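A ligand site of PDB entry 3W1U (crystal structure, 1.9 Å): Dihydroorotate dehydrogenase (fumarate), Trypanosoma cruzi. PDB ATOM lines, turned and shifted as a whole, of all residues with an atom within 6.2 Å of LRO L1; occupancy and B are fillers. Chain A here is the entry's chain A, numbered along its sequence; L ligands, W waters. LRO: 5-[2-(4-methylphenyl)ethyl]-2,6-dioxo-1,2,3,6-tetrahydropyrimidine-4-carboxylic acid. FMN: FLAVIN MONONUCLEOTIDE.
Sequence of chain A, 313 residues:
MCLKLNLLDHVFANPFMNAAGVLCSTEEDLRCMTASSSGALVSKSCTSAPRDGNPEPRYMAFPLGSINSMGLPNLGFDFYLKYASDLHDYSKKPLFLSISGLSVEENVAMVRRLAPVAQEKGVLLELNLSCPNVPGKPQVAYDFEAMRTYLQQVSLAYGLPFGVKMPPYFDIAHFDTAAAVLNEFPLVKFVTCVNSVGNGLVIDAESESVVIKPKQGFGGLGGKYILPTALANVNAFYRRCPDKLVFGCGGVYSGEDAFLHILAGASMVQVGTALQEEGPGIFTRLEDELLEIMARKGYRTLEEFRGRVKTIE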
ATOM      1  N   ALA A  20     -18.479  35.716 -17.909  1.00  0.00           N
ATOM      2  CA  ALA A  20     -18.266  34.463 -17.275  1.00  0.00           C
ATOM      3  C   ALA A  20     -18.482  33.331 -18.315  1.00  0.00           C
ATOM      4  O   ALA A  20     -19.399  33.387 -19.145  1.00  0.00           O
ATOM      5  CB  ALA A  20     -19.167  34.191 -16.048  1.00  0.00           C
ATOM      6  N   LYS A  44     -14.830  31.385 -14.275  1.00  0.00           N
ATOM      7  CA  LYS A  44     -15.892  30.493 -14.731  1.00  0.00           C
ATOM      8  C   LYS A  44     -16.819  30.163 -13.558  1.00  0.00           C
ATOM      9  O   LYS A  44     -16.346  29.772 -12.509  1.00  0.00           O
ATOM     10  CB  LYS A  44     -15.290  29.181 -15.238  1.00  0.00           C
ATOM     11  CG  LYS A  44     -16.297  28.072 -15.614  1.00  0.00           C
ATOM     12  CD  LYS A  44     -17.244  28.334 -16.775  1.00  0.00           C
ATOM     13  CE  LYS A  44     -18.410  27.373 -16.873  1.00  0.00           C
ATOM     14  NZ  LYS A  44     -19.350  27.584 -18.059  1.00  0.00           N
ATOM     15  N   SER A  45     -18.139  30.199 -13.846  1.00  0.00           N
ATOM     16  CA  SER A  45     -19.233  29.824 -12.918  1.00  0.00           C
ATOM     17  C   SER A  45     -18.899  28.453 -12.396  1.00  0.00           C
ATOM     18  O   SER A  45     -18.614  27.549 -13.164  1.00  0.00           O
ATOM     19  CB  SER A  45     -20.605  29.846 -13.546  1.00  0.00           C
ATOM     20  OG  SER A  45     -21.012  31.189 -13.791  1.00  0.00           O
ATOM     21  N   ASN A  54     -20.926  18.842 -20.524  1.00  0.00           N
ATOM     22  CA  ASN A  54     -21.584  18.008 -21.524  1.00  0.00           C
ATOM     23  C   ASN A  54     -20.636  17.506 -22.617  1.00  0.00           C
ATOM     24  O   ASN A  54     -19.545  18.043 -22.827  1.00  0.00           O
ATOM     25  CB  ASN A  54     -22.660  18.855 -22.214  1.00  0.00           C
ATOM     26  CG  ASN A  54     -23.854  19.089 -21.371  1.00  0.00           C
ATOM     27  OD1 ASN A  54     -24.165  18.286 -20.473  1.00  0.00           O
ATOM     28  ND2 ASN A  54     -24.554  20.163 -21.650  1.00  0.00           N
ATOM     29  N   ASN A  68     -24.273  27.633 -27.290  1.00  0.00           N
ATOM     30  CA  ASN A  68     -23.549  26.732 -26.374  1.00  0.00           C
ATOM     31  C   ASN A  68     -24.485  26.001 -25.460  1.00  0.00           C
ATOM     32  O   ASN A  68     -25.476  26.557 -24.998  1.00  0.00           O
ATOM     33  CB  ASN A  68     -22.488  27.514 -25.566  1.00  0.00           C
ATOM     34  CG  ASN A  68     -23.007  28.097 -24.281  1.00  0.00           C
ATOM     35  OD1 ASN A  68     -23.167  27.381 -23.271  1.00  0.00           O
ATOM     36  ND2 ASN A  68     -23.349  29.367 -24.309  1.00  0.00           N
ATOM     37  N   SER A  69     -24.123  24.773 -25.135  1.00  0.00           N
ATOM     38  CA  SER A  69     -24.709  24.031 -24.069  1.00  0.00           C
ATOM     39  C   SER A  69     -23.574  23.309 -23.397  1.00  0.00           C
ATOM     40  O   SER A  69     -23.465  22.094 -23.437  1.00  0.00           O
ATOM     41  CB  SER A  69     -25.828  23.048 -24.523  1.00  0.00           C
ATOM     42  OG  SER A  69     -27.018  23.734 -24.892  1.00  0.00           O
ATOM     43  N   MET A  70     -22.763  24.102 -22.684  1.00  0.00           N
ATOM     44  CA  MET A  70     -21.512  23.569 -22.136  1.00  0.00           C
ATOM     45  C   MET A  70     -21.755  22.568 -20.979  1.00  0.00           C
ATOM     46  O   MET A  70     -21.012  21.597 -20.765  1.00  0.00           O
ATOM     47  CB  MET A  70     -20.633  24.709 -21.629  1.00  0.00           C
ATOM     48  CG  MET A  70     -20.286  25.813 -22.585  1.00  0.00           C
ATOM     49  SD  MET A  70     -19.340  25.296 -23.966  1.00  0.00           S
ATOM     50  CE  MET A  70     -17.801  24.891 -23.191  1.00  0.00           C
ATOM     51  N   GLY A  71     -22.807  22.811 -20.204  1.00  0.00           N
ATOM     52  CA  GLY A  71     -23.128  21.953 -19.105  1.00  0.00           C
ATOM     53  C   GLY A  71     -22.310  22.292 -17.840  1.00  0.00           C
ATOM     54  O   GLY A  71     -22.001  21.397 -17.063  1.00  0.00           O
ATOM     55  N   LEU A  72     -21.946  23.555 -17.663  1.00  0.00           N
ATOM     56  CA  LEU A  72     -21.191  24.006 -16.520  1.00  0.00           C
ATOM     57  C   LEU A  72     -19.899  23.217 -16.195  1.00  0.00           C
ATOM     58  O   LEU A  72     -19.663  22.858 -15.049  1.00  0.00           O
ATOM     59  CB  LEU A  72     -22.076  23.964 -15.272  1.00  0.00           C
ATOM     60  CG  LEU A  72     -22.560  25.221 -14.579  1.00  0.00           C
ATOM     61  CD1 LEU A  72     -23.403  24.894 -13.337  1.00  0.00           C
ATOM     62  CD2 LEU A  72     -21.489  26.307 -14.413  1.00  0.00           C
ATOM     63  N   PRO A  73     -19.062  23.005 -17.178  1.00  0.00           N
ATOM     64  CA  PRO A  73     -17.788  22.356 -16.849  1.00  0.00           C
ATOM     65  C   PRO A  73     -16.924  23.349 -16.041  1.00  0.00           C
ATOM     66  O   PRO A  73     -16.934  24.529 -16.358  1.00  0.00           O
ATOM     67  CB  PRO A  73     -17.163  22.124 -18.186  1.00  0.00           C
ATOM     68  CG  PRO A  73     -17.691  23.215 -19.106  1.00  0.00           C
ATOM     69  CD  PRO A  73     -19.058  23.613 -18.512  1.00  0.00           C
ATOM     70  N   SER A 100     -22.381  29.220  -9.470  1.00  0.00           N
ATOM     71  CA  SER A 100     -23.599  28.759 -10.061  1.00  0.00           C
ATOM     72  C   SER A 100     -23.953  27.391  -9.516  1.00  0.00           C
ATOM     73  O   SER A 100     -24.035  26.339 -10.234  1.00  0.00           O
ATOM     74  CB  SER A 100     -23.381  28.792 -11.581  1.00  0.00           C
ATOM     75  OG  SER A 100     -24.536  28.271 -12.140  1.00  0.00           O
ATOM     76  N   ASN A 128     -24.758  33.555 -10.426  1.00  0.00           N
ATOM     77  CA  ASN A 128     -25.428  33.267 -11.659  1.00  0.00           C
ATOM     78  C   ASN A 128     -26.812  32.706 -11.365  1.00  0.00           C
ATOM     79  O   ASN A 128     -26.990  31.595 -10.899  1.00  0.00           O
ATOM     80  CB  ASN A 128     -24.568  32.319 -12.489  1.00  0.00           C
ATOM     81  CG  ASN A 128     -25.169  31.918 -13.809  1.00  0.00           C
ATOM     82  OD1 ASN A 128     -26.142  32.428 -14.243  1.00  0.00           O
ATOM     83  ND2 ASN A 128     -24.497  31.042 -14.476  1.00  0.00           N
ATOM     84  N   SER A 130     -29.032  32.064 -13.695  1.00  0.00           N
ATOM     85  CA  SER A 130     -29.417  31.086 -14.692  1.00  0.00           C
ATOM     86  C   SER A 130     -29.086  29.687 -14.221  1.00  0.00           C
ATOM     87  O   SER A 130     -29.214  28.786 -14.954  1.00  0.00           O
ATOM     88  CB  SER A 130     -28.823  31.325 -16.022  1.00  0.00           C
ATOM     89  OG  SER A 130     -29.259  32.524 -16.590  1.00  0.00           O
ATOM     90  N   CYS A 131     -28.665  29.502 -12.960  1.00  0.00           N
ATOM     91  CA  CYS A 131     -28.450  28.162 -12.472  1.00  0.00           C
ATOM     92  C   CYS A 131     -29.822  27.385 -12.746  1.00  0.00           C
ATOM     93  O   CYS A 131     -30.954  27.845 -12.553  1.00  0.00           O
ATOM     94  CB  CYS A 131     -28.009  28.135 -11.050  1.00  0.00           C
ATOM     95  SG  CYS A 131     -28.849  29.271  -9.942  1.00  0.00           S
ATOM     96  N   PRO A 132     -29.615  26.189 -13.460  1.00  0.00           N
ATOM     97  CA  PRO A 132     -30.774  25.305 -13.474  1.00  0.00           C
ATOM     98  C   PRO A 132     -31.153  24.967 -12.053  1.00  0.00           C
ATOM     99  O   PRO A 132     -30.325  25.005 -11.198  1.00  0.00           O
ATOM    100  CB  PRO A 132     -30.212  24.042 -14.117  1.00  0.00           C
ATOM    101  CG  PRO A 132     -29.400  24.551 -15.206  1.00  0.00           C
ATOM    102  CD  PRO A 132     -28.633  25.629 -14.531  1.00  0.00           C
ATOM    103  N   LYS A 165     -25.994  37.695 -12.070  1.00  0.00           N
ATOM    104  CA  LYS A 165     -26.017  37.524 -13.521  1.00  0.00           C
ATOM    105  C   LYS A 165     -27.408  37.059 -13.895  1.00  0.00           C
ATOM    106  O   LYS A 165     -27.902  36.003 -13.458  1.00  0.00           O
ATOM    107  CB  LYS A 165     -24.958  36.521 -13.951  1.00  0.00           C
ATOM    108  CG  LYS A 165     -25.043  36.162 -15.420  1.00  0.00           C
ATOM    109  CD  LYS A 165     -24.351  37.239 -16.222  1.00  0.00           C
ATOM    110  CE  LYS A 165     -23.971  36.791 -17.618  1.00  0.00           C
ATOM    111  NZ  LYS A 165     -22.763  36.001 -17.696  1.00  0.00           N
ATOM    112  N   ASN A 195     -27.092  37.153 -19.561  1.00  0.00           N
ATOM    113  CA  ASN A 195     -26.660  35.808 -19.925  1.00  0.00           C
ATOM    114  C   ASN A 195     -27.146  35.525 -21.352  1.00  0.00           C
ATOM    115  O   ASN A 195     -27.855  36.333 -21.993  1.00  0.00           O
ATOM    116  CB  ASN A 195     -27.218  34.730 -18.919  1.00  0.00           C
ATOM    117  CG  ASN A 195     -26.265  33.549 -18.734  1.00  0.00           C
ATOM    118  OD1 ASN A 195     -25.763  33.000 -19.702  1.00  0.00           O
ATOM    119  ND2 ASN A 195     -25.837  33.323 -17.507  1.00  0.00           N
ATOM    120  N   SER A 196     -26.817  34.346 -21.853  1.00  0.00           N
ATOM    121  CA  SER A 196     -27.296  33.950 -23.204  1.00  0.00           C
ATOM    122  C   SER A 196     -28.824  33.917 -23.378  1.00  0.00           C
ATOM    123  O   SER A 196     -29.608  33.722 -22.417  1.00  0.00           O
ATOM    124  CB  SER A 196     -26.607  32.590 -23.602  1.00  0.00           C
ATOM    125  OG  SER A 196     -26.804  31.614 -22.666  1.00  0.00           O
ATOM    126  N   LYS A 215     -28.743  18.353 -25.742  1.00  0.00           N
ATOM    127  CA  LYS A 215     -30.072  19.011 -25.793  1.00  0.00           C
ATOM    128  C   LYS A 215     -30.628  19.030 -27.220  1.00  0.00           C
ATOM    129  O   LYS A 215     -31.333  19.972 -27.600  1.00  0.00           O
ATOM    130  CB  LYS A 215     -29.966  20.443 -25.225  1.00  0.00           C
ATOM    131  CG  LYS A 215     -29.684  20.431 -23.742  1.00  0.00           C
ATOM    132  CD  LYS A 215     -29.627  21.831 -23.118  1.00  0.00           C
ATOM    133  CE  LYS A 215     -30.880  22.645 -23.403  1.00  0.00           C
ATOM    134  NZ  LYS A 215     -30.854  23.926 -22.617  1.00  0.00           N
ATOM    135  N   GLY A 220     -27.772  28.152 -25.594  1.00  0.00           N
ATOM    136  CA  GLY A 220     -27.864  29.572 -25.447  1.00  0.00           C
ATOM    137  C   GLY A 220     -27.093  30.329 -26.529  1.00  0.00           C
ATOM    138  O   GLY A 220     -26.023  29.950 -26.961  1.00  0.00           O
ATOM    139  N   LEU A 221     -27.699  31.426 -26.924  1.00  0.00           N
ATOM    140  CA  LEU A 221     -27.198  32.247 -28.034  1.00  0.00           C
ATOM    141  C   LEU A 221     -26.455  33.415 -27.481  1.00  0.00           C
ATOM    142  O   LEU A 221     -26.898  34.075 -26.536  1.00  0.00           O
ATOM    143  CB  LEU A 221     -28.317  32.805 -28.893  1.00  0.00           C
ATOM    144  CG  LEU A 221     -29.232  31.764 -29.504  1.00  0.00           C
ATOM    145  CD1 LEU A 221     -30.474  32.453 -30.102  1.00  0.00           C
ATOM    146  CD2 LEU A 221     -28.468  30.910 -30.476  1.00  0.00           C
HETATM  147  OAB LRO L   1     -23.718  25.825 -20.278  1.00  0.00           O
HETATM  148  CAN LRO L   1     -23.128  26.571 -19.522  1.00  0.00           C
HETATM  149  OAE LRO L   1     -22.191  26.152 -18.835  1.00  0.00           O
HETATM  150  CAQ LRO L   1     -23.602  27.944 -19.465  1.00  0.00           C
HETATM  151  NAL LRO L   1     -23.683  28.549 -20.723  1.00  0.00           N
HETATM  152  CAS LRO L   1     -24.219  29.891 -20.807  1.00  0.00           C
HETATM  153  OAC LRO L   1     -24.344  30.448 -21.890  1.00  0.00           O
HETATM  154  NAM LRO L   1     -24.612  30.541 -19.610  1.00  0.00           N
HETATM  155  CAT LRO L   1     -24.514  29.912 -18.345  1.00  0.00           C
HETATM  156  OAD LRO L   1     -24.869  30.543 -17.323  1.00  0.00           O
HETATM  157  CAR LRO L   1     -23.971  28.580 -18.292  1.00  0.00           C
HETATM  158  CAK LRO L   1     -23.860  27.929 -17.051  1.00  0.00           C
HETATM  159  CAJ LRO L   1     -25.251  27.668 -16.411  1.00  0.00           C
HETATM  160  CAP LRO L   1     -25.981  26.658 -17.114  1.00  0.00           C
HETATM  161  CAH LRO L   1     -26.993  27.078 -18.024  1.00  0.00           C
HETATM  162  CAF LRO L   1     -27.841  26.240 -18.808  1.00  0.00           C
HETATM  163  CAO LRO L   1     -27.659  24.867 -18.692  1.00  0.00           C
HETATM  164  CAA LRO L   1     -28.521  24.027 -19.542  1.00  0.00           C
HETATM  165  CAG LRO L   1     -26.605  24.406 -17.815  1.00  0.00           C
HETATM  166  CAI LRO L   1     -25.770  25.266 -17.007  1.00  0.00           C
HETATM  167  N1  FMN L   2     -22.531  32.903 -18.248  1.00  0.00           N
HETATM  168  C2  FMN L   2     -22.369  32.681 -16.905  1.00  0.00           C
HETATM  169  O2  FMN L   2     -22.915  33.491 -16.115  1.00  0.00           O
HETATM  170  N3  FMN L   2     -21.682  31.609 -16.395  1.00  0.00           N
HETATM  171  C4  FMN L   2     -21.107  30.704 -17.192  1.00  0.00           C
HETATM  172  O4  FMN L   2     -20.379  29.741 -16.813  1.00  0.00           O
HETATM  173  C4A FMN L   2     -21.126  30.956 -18.622  1.00  0.00           C
HETATM  174  N5  FMN L   2     -20.550  30.072 -19.437  1.00  0.00           N
HETATM  175  C5A FMN L   2     -20.521  30.364 -20.801  1.00  0.00           C
HETATM  176  C6  FMN L   2     -19.752  29.594 -21.661  1.00  0.00           C
HETATM  177  C7  FMN L   2     -19.710  29.876 -23.044  1.00  0.00           C
HETATM  178  C7M FMN L   2     -18.882  29.017 -23.925  1.00  0.00           C
HETATM  179  C8  FMN L   2     -20.373  31.049 -23.568  1.00  0.00           C
HETATM  180  C8M FMN L   2     -20.368  31.362 -25.024  1.00  0.00           C
HETATM  181  C9  FMN L   2     -21.153  31.808 -22.720  1.00  0.00           C
HETATM  182  C9A FMN L   2     -21.211  31.533 -21.362  1.00  0.00           C
HETATM  183  N10 FMN L   2     -21.970  32.331 -20.471  1.00  0.00           N
HETATM  184  C10 FMN L   2     -21.872  32.127 -19.121  1.00  0.00           C
HETATM  185  C1' FMN L   2     -22.688  33.489 -20.951  1.00  0.00           C
HETATM  186  C2' FMN L   2     -21.741  34.629 -21.202  1.00  0.00           C
HETATM  187  O2' FMN L   2     -21.223  35.006 -19.932  1.00  0.00           O
HETATM  188  C3' FMN L   2     -22.545  35.770 -21.799  1.00  0.00           C
HETATM  189  O3' FMN L   2     -23.526  36.139 -20.830  1.00  0.00           O
HETATM  190  C4' FMN L   2     -23.286  35.413 -23.100  1.00  0.00           C
HETATM  191  O4' FMN L   2     -22.382  34.642 -23.902  1.00  0.00           O
HETATM  192  C5' FMN L   2     -23.693  36.687 -23.888  1.00  0.00           C
HETATM  193  O5' FMN L   2     -22.587  37.550 -24.192  1.00  0.00           O
HETATM  194  P   FMN L   2     -21.869  37.651 -25.665  1.00  0.00           P
HETATM  195  O1P FMN L   2     -22.948  37.987 -26.617  1.00  0.00           O
HETATM  196  O2P FMN L   2     -21.505  36.204 -25.944  1.00  0.00           O
HETATM  197  O3P FMN L   2     -20.665  38.539 -25.519  1.00  0.00           O
HETATM  198  O   HOH W   1     -25.796  23.378 -21.010  1.00  0.00           O
HETATM  199  O   HOH W   2     -27.109  20.934 -19.896  1.00  0.00           O
HETATM  200  O   HOH W   3     -26.190  26.878 -21.929  1.00  0.00           O
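The side-chain amide oxygen (OD1) of Asn 195 lies within hydrogen-bond range of a nitrogen (NAM) of LRO L1 (2.7 Å). The side-chain amide nitrogen (ND2) of Asn 68 is in hydrogen-bond range of an oxygen (OAC) of LRO L1, 2.8 Å away. OG of Ser 196 sits at hydrogen-bond distance from OAC of LRO L1 (2.8 Å). OAE of LRO L1 is in hydrogen-bond range of N of Leu 72 (2.9 Å). An oxygen (OAD) of LRO L1 lies within hydrogen-bond range of the side-chain amide nitrogen (ND2) of Asn 128, at 2.9 Å. N of Met 70 sits at hydrogen-bond distance from OAB of LRO L1 (3.1 Å). An oxygen (OAB) of LRO L1 lies within hydrogen-bond range of the backbone NH (N) of Gly 71 (3.1 Å). The side-chain amino group (NZ) of Lys 44 lies within salt-bridge range of an oxygen (OAE) of LRO L1. O2 of FMN L2 is in hydrogen-bond range of ND2 of Asn 195 (3.2 Å). The side-chain amide nitrogen (ND2) of Asn 128 sits at hydrogen-bond distance from an oxygen (O2) of FMN L2, 3.3 Å away. O4 of FMN L2 is in hydrogen-bond range of NZ of Lys 44, at 2.7 Å. The side-chain hydroxyl (OG) of Ser 45 lies within hydrogen-bond range of a nitrogen (N3) of FMN L2 (2.7 Å). The side-chain amino group (NZ) of Lys 165 lies within hydrogen-bond range of an oxygen (O2') of FMN L2 (2.9 Å). N of Ala 20 lies within hydrogen-bond range of O2' of FMN L2 (3.5 Å). O of Ala 20 is in hydrogen-bond range of O2' of FMN L2, 2.6 Å away.
The side-chain amide oxygen (OD1) of Asn 195 is in hydrogen-bond range of the side-chain hydroxyl (OG) of Ser 196 (3.4 Å). ND2 of Asn 195 lies within hydrogen-bond range of OD1 of Asn 128 (3.4 Å). The backbone NH (N) of Met 70 sits close to the side-chain amide oxygen (OD1) of Asn 68, 3.4 Å away. O of Asn 68 lies within hydrogen-bond range of N of Gly 220. The side-chain amide oxygen (OD1) of Asn 128 sits at hydrogen-bond distance from the backbone NH (N) of Ser 130 (3.0 Å). O of Asn 128 lies within hydrogen-bond range of SG of Cys 131, at 3.1 Å. N of Asn 54 is in hydrogen-bond range of O of Met 70 (2.8 Å). The side-chain amide nitrogen of Asn 54 lies close to the backbone NH of Gly 71 (3.5 Å).
A nitrogen (NAM) of LRO L1 sits close to a nitrogen (N1) of FMN L2 (3.4 Å).
Merely in contact with LRO L1: Pro 132 and Lys 215. Within 4 Å of LRO L1: Lys 44, Asn 68, Met 70, Gly 71, Leu 72, Asn 128, Pro 132, Asn 195, Ser 196 and Lys 215. The nearest printed residue that does not touch LRO L1 is Ser 69 (4.01 Å).
Water W3 lies within hydrogen-bond range of an oxygen (OAB) of LRO L1 and the backbone carbonyl oxygen (O) of Asn 68. Water W1 lies within hydrogen-bond range of N of Gly 71 (3.1 Å) and OAB of LRO L1 (3.3 Å).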
